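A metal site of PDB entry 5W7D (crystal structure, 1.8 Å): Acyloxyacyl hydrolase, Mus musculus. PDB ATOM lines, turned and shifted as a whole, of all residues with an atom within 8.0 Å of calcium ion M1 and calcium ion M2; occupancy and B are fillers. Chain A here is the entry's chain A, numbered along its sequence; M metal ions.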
ATOM      1  N   PRO A 168      -0.370  16.746   9.037  1.00  0.00           N
ATOM      2  CA  PRO A 168      -0.209  16.479   7.597  1.00  0.00           C
ATOM      3  C   PRO A 168      -0.609  17.665   6.774  1.00  0.00           C
ATOM      4  O   PRO A 168      -1.566  18.378   7.074  1.00  0.00           O
ATOM      5  CB  PRO A 168      -1.122  15.286   7.332  1.00  0.00           C
ATOM      6  CG  PRO A 168      -2.061  15.252   8.470  1.00  0.00           C
ATOM      7  CD  PRO A 168      -1.327  15.812   9.650  1.00  0.00           C
ATOM      8  N   LYS A 170      -1.443  17.328   3.510  1.00  0.00           N
ATOM      9  CA  LYS A 170      -2.614  16.858   2.776  1.00  0.00           C
ATOM     10  C   LYS A 170      -3.631  16.296   3.774  1.00  0.00           C
ATOM     11  O   LYS A 170      -3.413  15.232   4.354  1.00  0.00           O
ATOM     12  CB  LYS A 170      -2.228  15.777   1.767  1.00  0.00           C
ATOM     13  CG  LYS A 170      -1.197  16.214   0.733  1.00  0.00           C
ATOM     14  CD  LYS A 170      -1.874  17.029  -0.358  1.00  0.00           C
ATOM     15  CE  LYS A 170      -0.931  17.304  -1.520  1.00  0.00           C
ATOM     16  NZ  LYS A 170      -1.436  18.409  -2.412  1.00  0.00           N
ATOM     17  N   ASP A 171      -4.729  17.014   3.968  1.00  0.00           N
ATOM     18  CA  ASP A 171      -5.689  16.653   5.004  1.00  0.00           C
ATOM     19  C   ASP A 171      -6.924  17.515   4.808  1.00  0.00           C
ATOM     20  O   ASP A 171      -7.124  18.517   5.488  1.00  0.00           O
ATOM     21  CB  ASP A 171      -5.062  16.828   6.382  1.00  0.00           C
ATOM     22  CG  ASP A 171      -6.019  16.495   7.539  1.00  0.00           C
ATOM     23  OD1 ASP A 171      -7.044  15.812   7.338  1.00  0.00           O
ATOM     24  OD2 ASP A 171      -5.717  16.922   8.672  1.00  0.00           O
ATOM     25  N   VAL A 172      -7.764  17.115   3.854  1.00  0.00           N
ATOM     26  CA  VAL A 172      -8.836  17.992   3.393  1.00  0.00           C
ATOM     27  C   VAL A 172      -9.803  18.318   4.526  1.00  0.00           C
ATOM     28  O   VAL A 172     -10.248  19.455   4.655  1.00  0.00           O
ATOM     29  CB  VAL A 172      -9.553  17.346   2.193  1.00  0.00           C
ATOM     30  CG1 VAL A 172     -10.868  18.108   1.856  1.00  0.00           C
ATOM     31  CG2 VAL A 172      -8.590  17.329   0.997  1.00  0.00           C
ATOM     32  N   ASP A 173     -10.106  17.338   5.396  1.00  0.00           N
ATOM     33  CA  ASP A 173     -11.084  17.528   6.457  1.00  0.00           C
ATOM     34  C   ASP A 173     -10.467  17.917   7.790  1.00  0.00           C
ATOM     35  O   ASP A 173     -11.202  18.074   8.764  1.00  0.00           O
ATOM     36  CB  ASP A 173     -11.949  16.250   6.627  1.00  0.00           C
ATOM     37  CG  ASP A 173     -11.152  15.014   7.023  1.00  0.00           C
ATOM     38  OD1 ASP A 173      -9.980  15.165   7.418  1.00  0.00           O
ATOM     39  OD2 ASP A 173     -11.717  13.901   6.945  1.00  0.00           O
ATOM     40  N   SER A 174      -9.150  18.105   7.844  1.00  0.00           N
ATOM     41  CA  SER A 174      -8.459  18.658   8.993  1.00  0.00           C
ATOM     42  C   SER A 174      -8.560  17.787  10.245  1.00  0.00           C
ATOM     43  O   SER A 174      -8.510  18.311  11.362  1.00  0.00           O
ATOM     44  CB  SER A 174      -8.951  20.069   9.319  1.00  0.00           C
ATOM     45  OG  SER A 174      -8.710  20.910   8.222  1.00  0.00           O
ATOM     46  N   ASP A 175      -8.664  16.470  10.106  1.00  0.00           N
ATOM     47  CA  ASP A 175      -8.696  15.619  11.289  1.00  0.00           C
ATOM     48  C   ASP A 175      -7.330  15.031  11.631  1.00  0.00           C
ATOM     49  O   ASP A 175      -7.248  14.150  12.492  1.00  0.00           O
ATOM     50  CB  ASP A 175      -9.755  14.514  11.143  1.00  0.00           C
ATOM     51  CG  ASP A 175      -9.478  13.568   9.998  1.00  0.00           C
ATOM     52  OD1 ASP A 175      -8.369  13.547   9.423  1.00  0.00           O
ATOM     53  OD2 ASP A 175     -10.423  12.834   9.682  1.00  0.00           O
ATOM     54  N   LYS A 176      -6.275  15.508  10.976  1.00  0.00           N
ATOM     55  CA  LYS A 176      -4.881  15.150  11.212  1.00  0.00           C
ATOM     56  C   LYS A 176      -4.522  13.761  10.695  1.00  0.00           C
ATOM     57  O   LYS A 176      -3.410  13.321  10.914  1.00  0.00           O
ATOM     58  CB  LYS A 176      -4.508  15.246  12.691  1.00  0.00           C
ATOM     59  CG  LYS A 176      -4.782  16.628  13.277  1.00  0.00           C
ATOM     60  CD  LYS A 176      -4.335  16.732  14.683  1.00  0.00           C
ATOM     61  CE  LYS A 176      -4.244  18.181  15.122  1.00  0.00           C
ATOM     62  NZ  LYS A 176      -5.583  18.801  15.137  1.00  0.00           N
ATOM     63  N   HIS A 177      -5.414  13.094   9.964  1.00  0.00           N
ATOM     64  CA  HIS A 177      -5.079  11.852   9.269  1.00  0.00           C
ATOM     65  C   HIS A 177      -5.154  12.077   7.758  1.00  0.00           C
ATOM     66  O   HIS A 177      -6.039  12.763   7.274  1.00  0.00           O
ATOM     67  CB  HIS A 177      -6.035  10.719   9.690  1.00  0.00           C
ATOM     68  CG  HIS A 177      -5.932  10.348  11.126  1.00  0.00           C
ATOM     69  ND1 HIS A 177      -5.153   9.299  11.569  1.00  0.00           N
ATOM     70  CD2 HIS A 177      -6.443  10.934  12.225  1.00  0.00           C
ATOM     71  CE1 HIS A 177      -5.226   9.223  12.884  1.00  0.00           C
ATOM     72  NE2 HIS A 177      -6.007  10.200  13.314  1.00  0.00           N
ATOM     73  N   SER A 178      -4.229  11.454   7.030  1.00  0.00           N
ATOM     74  CA  SER A 178      -4.000  11.749   5.612  1.00  0.00           C
ATOM     75  C   SER A 178      -4.222  10.519   4.752  1.00  0.00           C
ATOM     76  O   SER A 178      -4.201   9.379   5.239  1.00  0.00           O
ATOM     77  CB  SER A 178      -2.555  12.268   5.432  1.00  0.00           C
ATOM     78  OG  SER A 178      -2.292  12.751   4.121  1.00  0.00           O
ATOM     79  N   VAL A 179      -4.411  10.754   3.444  1.00  0.00           N
ATOM     80  CA  VAL A 179      -4.343   9.679   2.474  1.00  0.00           C
ATOM     81  C   VAL A 179      -3.003   9.621   1.774  1.00  0.00           C
ATOM     82  O   VAL A 179      -2.794   8.724   0.952  1.00  0.00           O
ATOM     83  CB  VAL A 179      -5.488   9.769   1.437  1.00  0.00           C
ATOM     84  CG1 VAL A 179      -6.845   9.786   2.177  1.00  0.00           C
ATOM     85  CG2 VAL A 179      -5.294  10.942   0.462  1.00  0.00           C
ATOM     86  N   GLY A 190      -2.464   6.447  11.455  1.00  0.00           N
ATOM     87  CA  GLY A 190      -3.345   5.676  10.598  1.00  0.00           C
ATOM     88  C   GLY A 190      -3.923   6.452   9.440  1.00  0.00           C
ATOM     89  O   GLY A 190      -4.313   7.626   9.581  1.00  0.00           O
ATOM     90  N   ARG A 191      -3.927   5.828   8.271  1.00  0.00           N
ATOM     91  CA  ARG A 191      -4.486   6.436   7.090  1.00  0.00           C
ATOM     92  C   ARG A 191      -5.972   6.747   7.264  1.00  0.00           C
ATOM     93  O   ARG A 191      -6.746   5.922   7.768  1.00  0.00           O
ATOM     94  CB  ARG A 191      -4.272   5.510   5.904  1.00  0.00           C
ATOM     95  CG  ARG A 191      -4.698   6.096   4.586  1.00  0.00           C
ATOM     96  CD  ARG A 191      -4.791   5.086   3.473  1.00  0.00           C
ATOM     97  NE  ARG A 191      -3.595   4.299   3.197  1.00  0.00           N
ATOM     98  CZ  ARG A 191      -2.940   4.253   2.032  1.00  0.00           C
ATOM     99  NH1 ARG A 191      -3.304   4.994   0.997  1.00  0.00           N
ATOM    100  NH2 ARG A 191      -1.894   3.450   1.902  1.00  0.00           N
ATOM    101  N   ASP A 192      -6.370   7.920   6.785  1.00  0.00           N
ATOM    102  CA  ASP A 192      -7.759   8.358   6.772  1.00  0.00           C
ATOM    103  C   ASP A 192      -8.542   7.591   5.719  1.00  0.00           C
ATOM    104  O   ASP A 192      -8.261   7.717   4.511  1.00  0.00           O
ATOM    105  CB  ASP A 192      -7.814   9.871   6.485  1.00  0.00           C
ATOM    106  CG  ASP A 192      -9.112  10.525   6.904  1.00  0.00           C
ATOM    107  OD1 ASP A 192     -10.054   9.784   7.197  1.00  0.00           O
ATOM    108  OD2 ASP A 192      -9.153  11.795   6.961  1.00  0.00           O
ATOM    109  N   CYS A 193      -9.565   6.857   6.153  1.00  0.00           N
ATOM    110  CA  CYS A 193     -10.431   6.142   5.205  1.00  0.00           C
ATOM    111  C   CYS A 193     -11.448   7.065   4.546  1.00  0.00           C
ATOM    112  O   CYS A 193     -11.979   6.733   3.473  1.00  0.00           O
ATOM    113  CB  CYS A 193     -11.109   4.951   5.927  1.00  0.00           C
ATOM    114  SG  CYS A 193     -12.095   5.326   7.464  1.00  0.00           S
ATOM    115  N   ASN A 194     -11.699   8.258   5.104  1.00  0.00           N
ATOM    116  CA  ASN A 194     -12.556   9.234   4.439  1.00  0.00           C
ATOM    117  C   ASN A 194     -12.044  10.636   4.781  1.00  0.00           C
ATOM    118  O   ASN A 194     -12.324  11.155   5.845  1.00  0.00           O
ATOM    119  CB  ASN A 194     -14.004   9.047   4.844  1.00  0.00           C
ATOM    120  CG  ASN A 194     -14.939   9.862   4.016  1.00  0.00           C
ATOM    121  OD1 ASN A 194     -14.562  10.880   3.416  1.00  0.00           O
ATOM    122  ND2 ASN A 194     -16.186   9.426   3.985  1.00  0.00           N
ATOM    123  N   ASP A 195     -11.279  11.202   3.867  1.00  0.00           N
ATOM    124  CA  ASP A 195     -10.685  12.513   4.064  1.00  0.00           C
ATOM    125  C   ASP A 195     -11.660  13.660   3.779  1.00  0.00           C
ATOM    126  O   ASP A 195     -11.239  14.821   3.843  1.00  0.00           O
ATOM    127  CB  ASP A 195      -9.433  12.609   3.184  1.00  0.00           C
ATOM    128  CG  ASP A 195      -8.503  13.722   3.590  1.00  0.00           C
ATOM    129  OD1 ASP A 195      -8.376  14.031   4.796  1.00  0.00           O
ATOM    130  OD2 ASP A 195      -7.854  14.285   2.687  1.00  0.00           O
ATOM    131  N   SER A 196     -12.940  13.350   3.493  1.00  0.00           N
ATOM    132  CA  SER A 196     -14.029  14.320   3.410  1.00  0.00           C
ATOM    133  C   SER A 196     -14.965  14.288   4.622  1.00  0.00           C
ATOM    134  O   SER A 196     -16.110  14.745   4.521  1.00  0.00           O
ATOM    135  CB  SER A 196     -14.856  14.081   2.153  1.00  0.00           C
ATOM    136  OG  SER A 196     -14.044  14.064   1.022  1.00  0.00           O
ATOM    137  N   ASP A 197     -14.538  13.710   5.740  1.00  0.00           N
ATOM    138  CA  ASP A 197     -15.396  13.610   6.908  1.00  0.00           C
ATOM    139  C   ASP A 197     -14.528  13.623   8.147  1.00  0.00           C
ATOM    140  O   ASP A 197     -13.876  12.618   8.465  1.00  0.00           O
ATOM    141  CB  ASP A 197     -16.265  12.355   6.851  1.00  0.00           C
ATOM    142  CG  ASP A 197     -17.327  12.337   7.932  1.00  0.00           C
ATOM    143  OD1 ASP A 197     -17.149  13.033   8.958  1.00  0.00           O
ATOM    144  OD2 ASP A 197     -18.346  11.639   7.759  1.00  0.00           O
ATOM    145  N   LYS A 198     -14.549  14.741   8.868  1.00  0.00           N
ATOM    146  CA  LYS A 198     -13.702  14.923  10.026  1.00  0.00           C
ATOM    147  C   LYS A 198     -14.121  14.067  11.214  1.00  0.00           C
ATOM    148  O   LYS A 198     -13.404  14.067  12.231  1.00  0.00           O
ATOM    149  CB  LYS A 198     -13.706  16.407  10.446  1.00  0.00           C
ATOM    150  CG  LYS A 198     -15.084  16.914  10.884  1.00  0.00           C
ATOM    151  CD  LYS A 198     -14.998  18.358  11.377  1.00  0.00           C
ATOM    152  CE  LYS A 198     -16.383  18.873  11.756  1.00  0.00           C
ATOM    153  NZ  LYS A 198     -16.360  20.278  12.281  1.00  0.00           N
ATOM    154  N   THR A 199     -15.255  13.359  11.125  1.00  0.00           N
ATOM    155  CA  THR A 199     -15.668  12.442  12.174  1.00  0.00           C
ATOM    156  C   THR A 199     -15.340  10.991  11.836  1.00  0.00           C
ATOM    157  O   THR A 199     -15.732  10.088  12.576  1.00  0.00           O
ATOM    158  CB  THR A 199     -17.179  12.561  12.470  1.00  0.00           C
ATOM    159  OG1 THR A 199     -17.925  12.060  11.346  1.00  0.00           O
ATOM    160  CG2 THR A 199     -17.562  14.000  12.748  1.00  0.00           C
ATOM    161  N   VAL A 200     -14.654  10.755  10.735  1.00  0.00           N
ATOM    162  CA  VAL A 200     -14.198   9.426  10.307  1.00  0.00           C
ATOM    163  C   VAL A 200     -12.673   9.458  10.349  1.00  0.00           C
ATOM    164  O   VAL A 200     -12.053  10.163   9.552  1.00  0.00           O
ATOM    165  CB  VAL A 200     -14.702   9.066   8.905  1.00  0.00           C
ATOM    166  CG1 VAL A 200     -14.028   7.794   8.381  1.00  0.00           C
ATOM    167  CG2 VAL A 200     -16.231   8.936   8.921  1.00  0.00           C
ATOM    168  N   TYR A 201     -12.070   8.660  11.232  1.00  0.00           N
ATOM    169  CA  TYR A 201     -10.624   8.567  11.381  1.00  0.00           C
ATOM    170  C   TYR A 201     -10.305   7.429  12.353  1.00  0.00           C
ATOM    171  O   TYR A 201     -11.163   7.043  13.155  1.00  0.00           O
ATOM    172  CB  TYR A 201     -10.030   9.890  11.898  1.00  0.00           C
ATOM    173  CG  TYR A 201     -10.663  10.396  13.176  1.00  0.00           C
ATOM    174  CD1 TYR A 201     -10.295   9.874  14.405  1.00  0.00           C
ATOM    175  CD2 TYR A 201     -11.626  11.400  13.158  1.00  0.00           C
ATOM    176  CE1 TYR A 201     -10.873  10.304  15.571  1.00  0.00           C
ATOM    177  CE2 TYR A 201     -12.205  11.842  14.315  1.00  0.00           C
ATOM    178  CZ  TYR A 201     -11.826  11.298  15.527  1.00  0.00           C
ATOM    179  OH  TYR A 201     -12.417  11.743  16.678  1.00  0.00           O
ATOM    180  N   PRO A 202      -9.069   6.929  12.335  1.00  0.00           N
ATOM    181  CA  PRO A 202      -8.676   5.849  13.263  1.00  0.00           C
ATOM    182  C   PRO A 202      -8.720   6.281  14.718  1.00  0.00           C
ATOM    183  O   PRO A 202      -8.292   7.382  15.076  1.00  0.00           O
ATOM    184  CB  PRO A 202      -7.252   5.508  12.818  1.00  0.00           C
ATOM    185  CG  PRO A 202      -7.135   6.054  11.443  1.00  0.00           C
ATOM    186  CD  PRO A 202      -7.988   7.261  11.396  1.00  0.00           C
ATOM    187  N   GLN A 213     -21.066   2.751   7.274  1.00  0.00           N
ATOM    188  CA  GLN A 213     -19.765   3.298   6.962  1.00  0.00           C
ATOM    189  C   GLN A 213     -18.778   2.811   8.019  1.00  0.00           C
ATOM    190  O   GLN A 213     -19.139   2.626   9.188  1.00  0.00           O
ATOM    191  CB  GLN A 213     -19.726   4.848   6.906  1.00  0.00           C
ATOM    192  CG  GLN A 213     -18.276   5.402   6.784  1.00  0.00           C
ATOM    193  CD  GLN A 213     -18.121   6.872   6.280  1.00  0.00           C
ATOM    194  OE1 GLN A 213     -17.146   7.209   5.573  1.00  0.00           O
ATOM    195  NE2 GLN A 213     -19.061   7.747   6.687  1.00  0.00           N
ATOM    196  N   SER A 215     -16.594   3.985  10.194  1.00  0.00           N
ATOM    197  CA  SER A 215     -16.320   5.302  10.758  1.00  0.00           C
ATOM    198  C   SER A 215     -14.991   5.381  11.486  1.00  0.00           C
ATOM    199  O   SER A 215     -14.478   6.486  11.673  1.00  0.00           O
ATOM    200  CB  SER A 215     -17.440   5.746  11.703  1.00  0.00           C
ATOM    201  OG  SER A 215     -17.410   5.040  12.945  1.00  0.00           O
ATOM    202  N   CYS A 217     -12.186   3.435  10.575  1.00  0.00           N
ATOM    203  CA  CYS A 217     -11.116   3.063   9.658  1.00  0.00           C
ATOM    204  C   CYS A 217     -10.438   1.745  10.042  1.00  0.00           C
ATOM    205  O   CYS A 217      -9.317   1.453   9.555  1.00  0.00           O
ATOM    206  CB  CYS A 217     -10.063   4.173   9.553  1.00  0.00           C
ATOM    207  SG  CYS A 217     -10.792   5.772   9.083  1.00  0.00           S
HETATM  208 CA    CA M   1     -11.510  11.784   7.951  1.00  0.00          CA
HETATM  209 CA    CA M   2      -8.082  13.789   7.095  1.00  0.00          CA
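The backbone NH (N) of Asp 192 sits at hydrogen-bond distance from the backbone carbonyl oxygen (O) of Ser 178 (3.0 Å). The side-chain carboxylate of Asp 171 lies close to the backbone NH of Ser 174. The side-chain carboxylate (OD2) of Asp 171 is in hydrogen-bond range of the backbone NH (N) of Lys 176, 2.8 Å away. The backbone carbonyl oxygen (O) of Gly 190 is in hydrogen-bond range of a ring nitrogen (ND1) of His 177 (2.7 Å). OD2 of Asp 195 sits at hydrogen-bond distance from N of Val 172 (3.1 Å). The side-chain amide nitrogen (ND2) of Asn 194 lies within hydrogen-bond range of the side-chain amide oxygen (OE1) of Gln 213. OD1 of Asp 197 lies within hydrogen-bond range of OG1 of Thr 199, at 2.7 Å. The side-chain sulfur of Cys 193 forms a disulfide with the side-chain sulfur of Cys 217 (2.1 Å).
Six residues have an atom within 4 Å of calcium ion M1: Asp 173, Asp 175, Asp 192, Asn 194, Asp 197 and Val 200.
Six residues have an atom within 4 Å of calcium ion M2: Asp 171, Asp 173, Asp 175, His 177, Asp 192 and Asp 195. The nearest printed residue that does not touch calcium ion M2 is Ser 178 (4.5 Å).
Calcium ion M1 is bound by OD2 of Asp 175, O of Val 200, O of Asn 194, OD2 of Asp 173, OD2 of Asp 192, O of Asp 197 and OD1 of Asp 192.
Calcium ion M2 is bound by the side-chain carboxylate (OD2) of Asp 192 (2.3 Å), the side-chain carboxylate (OD1) of Asp 171 (2.3 Å), the backbone carbonyl oxygen (O) of His 177 (2.3 Å), the side-chain carboxylate (OD1) of Asp 195 (2.3 Å), the side-chain carboxylate (OD1) of Asp 175 (2.4 Å) and the side-chain carboxylate (OD1) of Asp 173 (2.4 Å). Calcium ion M2 has six donor atoms within binding distance.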
